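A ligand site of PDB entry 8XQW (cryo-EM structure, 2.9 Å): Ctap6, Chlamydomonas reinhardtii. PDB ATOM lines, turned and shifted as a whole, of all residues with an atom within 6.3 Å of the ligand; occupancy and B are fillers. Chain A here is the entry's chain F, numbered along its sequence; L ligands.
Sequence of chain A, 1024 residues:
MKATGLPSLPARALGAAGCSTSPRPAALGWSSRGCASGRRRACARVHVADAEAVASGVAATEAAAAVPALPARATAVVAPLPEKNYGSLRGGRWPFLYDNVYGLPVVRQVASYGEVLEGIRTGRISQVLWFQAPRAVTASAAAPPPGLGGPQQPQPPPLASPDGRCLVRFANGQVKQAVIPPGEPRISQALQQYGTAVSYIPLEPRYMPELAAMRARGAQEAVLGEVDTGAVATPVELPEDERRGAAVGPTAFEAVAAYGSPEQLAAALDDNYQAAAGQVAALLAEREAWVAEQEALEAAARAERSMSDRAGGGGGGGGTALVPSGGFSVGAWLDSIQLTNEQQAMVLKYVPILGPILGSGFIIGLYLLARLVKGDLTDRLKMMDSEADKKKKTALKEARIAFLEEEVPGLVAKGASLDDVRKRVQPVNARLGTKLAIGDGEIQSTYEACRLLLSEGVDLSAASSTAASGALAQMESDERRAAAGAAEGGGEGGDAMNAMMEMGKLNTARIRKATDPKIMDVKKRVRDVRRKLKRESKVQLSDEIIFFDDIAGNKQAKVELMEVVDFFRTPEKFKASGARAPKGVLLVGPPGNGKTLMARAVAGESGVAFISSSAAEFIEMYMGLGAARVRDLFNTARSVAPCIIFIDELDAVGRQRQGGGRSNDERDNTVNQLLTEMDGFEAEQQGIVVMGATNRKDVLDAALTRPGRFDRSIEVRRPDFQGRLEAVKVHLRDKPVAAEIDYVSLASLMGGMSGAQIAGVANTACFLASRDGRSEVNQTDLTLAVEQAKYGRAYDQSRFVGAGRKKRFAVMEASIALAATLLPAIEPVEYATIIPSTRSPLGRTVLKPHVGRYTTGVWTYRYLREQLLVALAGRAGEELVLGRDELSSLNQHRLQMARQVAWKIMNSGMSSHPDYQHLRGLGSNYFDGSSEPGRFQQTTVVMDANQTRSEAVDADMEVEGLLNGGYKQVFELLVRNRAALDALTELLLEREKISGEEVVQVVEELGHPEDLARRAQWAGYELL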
ATOM      1  N   ASP A 550      21.189   5.700  36.952  1.00  0.00           N
ATOM      2  CA  ASP A 550      22.366   5.514  36.110  1.00  0.00           C
ATOM      3  C   ASP A 550      22.569   6.696  35.163  1.00  0.00           C
ATOM      4  O   ASP A 550      23.706   6.937  34.737  1.00  0.00           O
ATOM      5  CB  ASP A 550      22.231   4.207  35.337  1.00  0.00           C
ATOM      6  CG  ASP A 550      23.567   3.657  34.861  1.00  0.00           C
ATOM      7  OD1 ASP A 550      24.402   4.434  34.333  1.00  0.00           O
ATOM      8  OD2 ASP A 550      23.787   2.446  34.993  1.00  0.00           O
ATOM      9  N   ILE A 551      21.523   7.441  34.835  1.00  0.00           N
ATOM     10  CA  ILE A 551      21.625   8.633  34.022  1.00  0.00           C
ATOM     11  C   ILE A 551      22.011   9.795  34.922  1.00  0.00           C
ATOM     12  O   ILE A 551      21.727   9.792  36.133  1.00  0.00           O
ATOM     13  CB  ILE A 551      20.314   8.956  33.270  1.00  0.00           C
ATOM     14  CG1 ILE A 551      19.533   7.681  32.952  1.00  0.00           C
ATOM     15  CG2 ILE A 551      20.617   9.708  31.976  1.00  0.00           C
ATOM     16  CD1 ILE A 551      20.250   6.738  32.011  1.00  0.00           C
ATOM     17  N   ALA A 552      22.660  10.799  34.346  1.00  0.00           N
ATOM     18  CA  ALA A 552      23.166  11.949  35.087  1.00  0.00           C
ATOM     19  C   ALA A 552      22.445  13.205  34.628  1.00  0.00           C
ATOM     20  O   ALA A 552      22.255  13.415  33.435  1.00  0.00           O
ATOM     21  CB  ALA A 552      24.669  12.111  34.890  1.00  0.00           C
ATOM     22  N   GLY A 553      22.044  14.028  35.591  1.00  0.00           N
ATOM     23  CA  GLY A 553      21.462  15.314  35.282  1.00  0.00           C
ATOM     24  C   GLY A 553      20.132  15.188  34.550  1.00  0.00           C
ATOM     25  O   GLY A 553      19.358  14.258  34.771  1.00  0.00           O
ATOM     26  N   ASN A 554      19.875  16.146  33.668  1.00  0.00           N
ATOM     27  CA  ASN A 554      18.655  16.205  32.877  1.00  0.00           C
ATOM     28  C   ASN A 554      17.438  16.143  33.795  1.00  0.00           C
ATOM     29  O   ASN A 554      16.447  15.458  33.508  1.00  0.00           O
ATOM     30  CB  ASN A 554      18.614  15.092  31.844  1.00  0.00           C
ATOM     31  CG  ASN A 554      19.935  14.894  31.149  1.00  0.00           C
ATOM     32  OD1 ASN A 554      20.592  15.856  30.756  1.00  0.00           O
ATOM     33  ND2 ASN A 554      20.337  13.640  30.984  1.00  0.00           N
ATOM     34  N   LYS A 558      14.187  13.724  33.465  1.00  0.00           N
ATOM     35  CA  LYS A 558      13.743  12.757  34.498  1.00  0.00           C
ATOM     36  C   LYS A 558      12.304  13.126  34.903  1.00  0.00           C
ATOM     37  O   LYS A 558      11.394  12.348  34.578  1.00  0.00           O
ATOM     38  CB  LYS A 558      14.678  12.786  35.709  1.00  0.00           C
ATOM     39  CG  LYS A 558      16.162  12.805  35.376  1.00  0.00           C
ATOM     40  CD  LYS A 558      16.610  11.763  34.365  1.00  0.00           C
ATOM     41  CE  LYS A 558      17.681  10.868  34.914  1.00  0.00           C
ATOM     42  NZ  LYS A 558      18.924  11.596  35.130  1.00  0.00           N
ATOM     43  N   PRO A 590      21.568  17.749  21.143  1.00  0.00           N
ATOM     44  CA  PRO A 590      22.737  17.428  20.351  1.00  0.00           C
ATOM     45  C   PRO A 590      23.105  15.957  20.508  1.00  0.00           C
ATOM     46  O   PRO A 590      22.871  15.363  21.583  1.00  0.00           O
ATOM     47  CB  PRO A 590      23.830  18.334  20.932  1.00  0.00           C
ATOM     48  CG  PRO A 590      23.102  19.391  21.689  1.00  0.00           C
ATOM     49  CD  PRO A 590      21.866  18.727  22.204  1.00  0.00           C
ATOM     50  N   PRO A 591      23.755  15.287  19.528  1.00  0.00           N
ATOM     51  CA  PRO A 591      24.184  13.901  19.731  1.00  0.00           C
ATOM     52  C   PRO A 591      25.323  13.776  20.735  1.00  0.00           C
ATOM     53  O   PRO A 591      26.059  14.750  20.957  1.00  0.00           O
ATOM     54  CB  PRO A 591      24.627  13.448  18.339  1.00  0.00           C
ATOM     55  CG  PRO A 591      25.101  14.719  17.678  1.00  0.00           C
ATOM     56  CD  PRO A 591      24.114  15.752  18.164  1.00  0.00           C
ATOM     57  N   GLY A 592      25.457  12.592  21.343  1.00  0.00           N
ATOM     58  CA  GLY A 592      26.517  12.361  22.355  1.00  0.00           C
ATOM     59  C   GLY A 592      26.004  12.565  23.773  1.00  0.00           C
ATOM     60  O   GLY A 592      26.644  12.062  24.713  1.00  0.00           O
ATOM     61  N   ASN A 593      24.885  13.275  23.921  1.00  0.00           N
ATOM     62  CA  ASN A 593      24.277  13.500  25.252  1.00  0.00           C
ATOM     63  C   ASN A 593      23.383  12.312  25.609  1.00  0.00           C
ATOM     64  O   ASN A 593      22.498  12.489  26.489  1.00  0.00           O
ATOM     65  CB  ASN A 593      23.553  14.842  25.317  1.00  0.00           C
ATOM     66  CG  ASN A 593      24.516  16.001  25.276  1.00  0.00           C
ATOM     67  OD1 ASN A 593      25.616  15.915  25.816  1.00  0.00           O
ATOM     68  ND2 ASN A 593      24.108  17.096  24.640  1.00  0.00           N
ATOM     69  N   GLY A 594      23.583  11.152  24.978  1.00  0.00           N
ATOM     70  CA  GLY A 594      22.851   9.908  25.337  1.00  0.00           C
ATOM     71  C   GLY A 594      21.360  10.091  25.375  1.00  0.00           C
ATOM     72  O   GLY A 594      20.796  10.168  26.488  1.00  0.00           O
ATOM     73  N   LYS A 595      20.730  10.126  24.206  1.00  0.00           N
ATOM     74  CA  LYS A 595      19.252  10.218  24.143  1.00  0.00           C
ATOM     75  C   LYS A 595      18.725   8.803  23.894  1.00  0.00           C
ATOM     76  O   LYS A 595      17.576   8.684  23.416  1.00  0.00           O
ATOM     77  CB  LYS A 595      18.839  11.184  23.039  1.00  0.00           C
ATOM     78  CG  LYS A 595      19.078  12.658  23.359  1.00  0.00           C
ATOM     79  CD  LYS A 595      18.482  13.619  22.338  1.00  0.00           C
ATOM     80  CE  LYS A 595      18.586  13.101  20.944  1.00  0.00           C
ATOM     81  NZ  LYS A 595      19.543  13.867  20.151  1.00  0.00           N
ATOM     82  N   THR A 596      19.536   7.783  24.178  1.00  0.00           N
ATOM     83  CA  THR A 596      19.110   6.380  23.971  1.00  0.00           C
ATOM     84  C   THR A 596      18.940   5.737  25.321  1.00  0.00           C
ATOM     85  O   THR A 596      17.805   5.375  25.658  1.00  0.00           O
ATOM     86  CB  THR A 596      20.143   5.650  23.120  1.00  0.00           C
ATOM     87  OG1 THR A 596      21.377   5.792  23.823  1.00  0.00           O
ATOM     88  CG2 THR A 596      20.261   6.231  21.725  1.00  0.00           C
ATOM     89  N   LEU A 597      20.023   5.608  26.092  1.00  0.00           N
ATOM     90  CA  LEU A 597      19.932   5.023  27.408  1.00  0.00           C
ATOM     91  C   LEU A 597      18.849   5.659  28.270  1.00  0.00           C
ATOM     92  O   LEU A 597      18.390   5.019  29.215  1.00  0.00           O
ATOM     93  CB  LEU A 597      21.295   5.084  28.116  1.00  0.00           C
ATOM     94  CG  LEU A 597      22.079   6.391  28.138  1.00  0.00           C
ATOM     95  CD1 LEU A 597      22.704   6.634  29.495  1.00  0.00           C
ATOM     96  CD2 LEU A 597      23.158   6.344  27.066  1.00  0.00           C
ATOM     97  N   MET A 598      18.385   6.864  27.937  1.00  0.00           N
ATOM     98  CA  MET A 598      17.222   7.408  28.638  1.00  0.00           C
ATOM     99  C   MET A 598      15.961   6.646  28.270  1.00  0.00           C
ATOM    100  O   MET A 598      15.125   6.344  29.132  1.00  0.00           O
ATOM    101  CB  MET A 598      17.068   8.896  28.314  1.00  0.00           C
ATOM    102  CG  MET A 598      16.319   9.673  29.392  1.00  0.00           C
ATOM    103  SD  MET A 598      16.309  11.446  29.088  1.00  0.00           S
ATOM    104  CE  MET A 598      17.781  11.626  28.075  1.00  0.00           C
ATOM    105  N   ASP A 648      15.487   5.715  16.374  1.00  0.00           N
ATOM    106  CA  ASP A 648      16.549   6.670  16.118  1.00  0.00           C
ATOM    107  C   ASP A 648      16.467   7.168  14.675  1.00  0.00           C
ATOM    108  O   ASP A 648      15.591   6.769  13.900  1.00  0.00           O
ATOM    109  CB  ASP A 648      17.924   6.040  16.343  1.00  0.00           C
ATOM    110  CG  ASP A 648      17.998   5.259  17.629  1.00  0.00           C
ATOM    111  OD1 ASP A 648      17.186   4.327  17.808  1.00  0.00           O
ATOM    112  OD2 ASP A 648      18.877   5.568  18.462  1.00  0.00           O
ATOM    113  N   ALA A 693      14.219   9.811  18.647  1.00  0.00           N
ATOM    114  CA  ALA A 693      15.394  10.627  18.899  1.00  0.00           C
ATOM    115  C   ALA A 693      15.782  11.355  17.618  1.00  0.00           C
ATOM    116  O   ALA A 693      16.032  10.714  16.590  1.00  0.00           O
ATOM    117  CB  ALA A 693      16.562   9.778  19.417  1.00  0.00           C
ATOM    118  N   ASN A 695      18.026  15.129  16.252  1.00  0.00           N
ATOM    119  CA  ASN A 695      18.877  16.234  16.668  1.00  0.00           C
ATOM    120  C   ASN A 695      18.138  17.563  16.606  1.00  0.00           C
ATOM    121  O   ASN A 695      18.225  18.376  17.539  1.00  0.00           O
ATOM    122  CB  ASN A 695      20.136  16.292  15.798  1.00  0.00           C
ATOM    123  CG  ASN A 695      20.781  14.939  15.624  1.00  0.00           C
ATOM    124  OD1 ASN A 695      20.726  14.336  14.550  1.00  0.00           O
ATOM    125  ND2 ASN A 695      21.404  14.432  16.683  1.00  0.00           N
ATOM    126  N   VAL A 716      17.460  17.807  25.620  1.00  0.00           N
ATOM    127  CA  VAL A 716      18.602  17.180  26.272  1.00  0.00           C
ATOM    128  C   VAL A 716      19.817  18.016  25.898  1.00  0.00           C
ATOM    129  O   VAL A 716      20.420  17.804  24.842  1.00  0.00           O
ATOM    130  CB  VAL A 716      18.789  15.713  25.855  1.00  0.00           C
ATOM    131  CG1 VAL A 716      20.058  15.151  26.468  1.00  0.00           C
ATOM    132  CG2 VAL A 716      17.589  14.897  26.280  1.00  0.00           C
ATOM    133  N   ALA A 727      27.957  13.385  36.603  1.00  0.00           N
ATOM    134  CA  ALA A 727      28.252  12.492  35.501  1.00  0.00           C
ATOM    135  C   ALA A 727      29.678  11.978  35.536  1.00  0.00           C
ATOM    136  O   ALA A 727      29.933  10.863  35.071  1.00  0.00           O
ATOM    137  CB  ALA A 727      27.983  13.196  34.173  1.00  0.00           C
ATOM    138  N   VAL A 730      29.859   9.324  38.733  1.00  0.00           N
ATOM    139  CA  VAL A 730      29.227   8.038  38.474  1.00  0.00           C
ATOM    140  C   VAL A 730      30.051   7.239  37.461  1.00  0.00           C
ATOM    141  O   VAL A 730      29.793   6.056  37.239  1.00  0.00           O
ATOM    142  CB  VAL A 730      27.774   8.217  38.001  1.00  0.00           C
ATOM    143  CG1 VAL A 730      26.990   9.000  39.026  1.00  0.00           C
ATOM    144  CG2 VAL A 730      27.741   8.909  36.647  1.00  0.00           C
ATOM    145  N   HIS A 731      31.047   7.868  36.848  1.00  0.00           N
ATOM    146  CA  HIS A 731      31.904   7.222  35.865  1.00  0.00           C
ATOM    147  C   HIS A 731      33.250   6.789  36.443  1.00  0.00           C
ATOM    148  O   HIS A 731      34.203   6.591  35.683  1.00  0.00           O
ATOM    149  CB  HIS A 731      32.123   8.153  34.674  1.00  0.00           C
ATOM    150  CG  HIS A 731      31.329   7.780  33.461  1.00  0.00           C
ATOM    151  ND1 HIS A 731      31.386   6.521  32.902  1.00  0.00           N
ATOM    152  CD2 HIS A 731      30.466   8.493  32.703  1.00  0.00           C
ATOM    153  CE1 HIS A 731      30.594   6.472  31.850  1.00  0.00           C
ATOM    154  NE2 HIS A 731      30.027   7.662  31.702  1.00  0.00           N
ATOM    155  N   GLY A 755      28.624  14.251  27.318  1.00  0.00           N
ATOM    156  CA  GLY A 755      28.831  13.108  28.188  1.00  0.00           C
ATOM    157  C   GLY A 755      29.785  12.077  27.618  1.00  0.00           C
ATOM    158  O   GLY A 755      30.657  11.563  28.329  1.00  0.00           O
ATOM    159  N   ALA A 756      29.632  11.771  26.323  1.00  0.00           N
ATOM    160  CA  ALA A 756      30.544  10.833  25.682  1.00  0.00           C
ATOM    161  C   ALA A 756      31.983  11.299  25.779  1.00  0.00           C
ATOM    162  O   ALA A 756      32.897  10.489  25.879  1.00  0.00           O
ATOM    163  CB  ALA A 756      30.144  10.632  24.223  1.00  0.00           C
ATOM    164  N   ALA A 759      33.212  10.400  29.272  1.00  0.00           N
ATOM    165  CA  ALA A 759      33.542   8.977  29.291  1.00  0.00           C
ATOM    166  C   ALA A 759      34.857   8.717  28.557  1.00  0.00           C
ATOM    167  O   ALA A 759      35.677   7.900  29.010  1.00  0.00           O
ATOM    168  CB  ALA A 759      32.411   8.162  28.674  1.00  0.00           C
HETATM  169  P1  LIG L   1      25.244   8.967  18.748  1.00  0.00           P
HETATM  170  O1  LIG L   1      24.551   8.196  17.673  1.00  0.00           O
HETATM  171  O2  LIG L   1      26.328   9.900  18.080  1.00  0.00           O
HETATM  172  O3  LIG L   1      25.952   7.967  19.748  1.00  0.00           O
HETATM  173  P2  LIG L   1      23.480   9.047  20.891  1.00  0.00           P
HETATM  174  O4  LIG L   1      22.233   9.734  21.349  1.00  0.00           O
HETATM  175  O5  LIG L   1      23.134   7.597  20.440  1.00  0.00           O
HETATM  176  N1  LIG L   1      24.124   9.907  19.597  1.00  0.00           N
HETATM  177  P3  LIG L   1      24.725   7.602  22.806  1.00  0.00           P
HETATM  178  O6  LIG L   1      25.331   6.628  21.870  1.00  0.00           O
HETATM  179  O7  LIG L   1      23.362   7.176  23.344  1.00  0.00           O
HETATM  180  O8  LIG L   1      24.493   8.989  22.076  1.00  0.00           O
HETATM  181  O9  LIG L   1      25.766   7.880  23.969  1.00  0.00           O
HETATM  182  C1  LIG L   1      26.325   6.790  24.747  1.00  0.00           C
HETATM  183  C2  LIG L   1      27.453   7.299  25.607  1.00  0.00           C
HETATM  184  O10 LIG L   1      27.119   8.606  26.122  1.00  0.00           O
HETATM  185  C3  LIG L   1      27.783   6.433  26.825  1.00  0.00           C
HETATM  186  O11 LIG L   1      29.191   6.404  27.039  1.00  0.00           O
HETATM  187  C4  LIG L   1      27.058   7.151  27.961  1.00  0.00           C
HETATM  188  O12 LIG L   1      27.720   6.957  29.204  1.00  0.00           O
HETATM  189  C5  LIG L   1      27.201   8.612  27.539  1.00  0.00           C
HETATM  190  N2  LIG L   1      26.177   9.500  28.055  1.00  0.00           N
HETATM  191  C6  LIG L   1      25.355  10.311  27.323  1.00  0.00           C
HETATM  192  N3  LIG L   1      24.509  11.016  28.041  1.00  0.00           N
HETATM  193  C7  LIG L   1      24.813  10.649  29.340  1.00  0.00           C
HETATM  194  C8  LIG L   1      24.283  11.043  30.586  1.00  0.00           C
HETATM  195  N4  LIG L   1      23.293  11.931  30.726  1.00  0.00           N
HETATM  196  N5  LIG L   1      24.802  10.486  31.699  1.00  0.00           N
HETATM  197  C9  LIG L   1      25.794   9.598  31.576  1.00  0.00           C
HETATM  198  N6  LIG L   1      26.372   9.143  30.461  1.00  0.00           N
HETATM  199  C10 LIG L   1      25.831   9.716  29.375  1.00  0.00           C
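The backbone NH (N) of Gly 592 sits close to a nitrogen (N1) of the ligand (3.5 Å).
O of Asn 593 lies close to N3 of the ligand.
Residues that only touch the ligand: Ile 551, Pro 591 and Leu 597.
Hydrophobic or aromatic side chains that line the ligand: Ile 551, Ala 552, Pro 591, Leu 597 and His 731.
Within 4 Å of the ligand: Ile 551, Ala 552, Asn 554, Pro 591, Gly 592, Asn 593, Gly 594, Lys 595, Thr 596, Leu 597 and His 731.
The side-chain hydroxyl (OG1) of Thr 596 lies within hydrogen-bond range of an oxygen (O7) of the ligand (2.5 Å).
N of Gly 594 sits close to N3 of the ligand (3.2 Å).
The backbone NH (N) of Lys 595 sits at hydrogen-bond distance from an oxygen (O4) of the ligand (3.3 Å).
N of Ala 552 is in hydrogen-bond range of N5 of the ligand (3.4 Å).
O of Ala 552 is in hydrogen-bond range of N4 of the ligand, at 3.3 Å.
ND2 of Asn 554 lies close to N4 of the ligand.
A ring nitrogen (NE2) of His 731 lies within hydrogen-bond range of an oxygen (O12) of the ligand (3.5 Å).
O of Ala 552 sits at hydrogen-bond distance from ND2 of Asn 554.
N of Ala 756 is in hydrogen-bond range of O of Gly 592, 3.4 Å away.
O of Ile 551 sits at hydrogen-bond distance from NZ of Lys 558 (3.5 Å).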
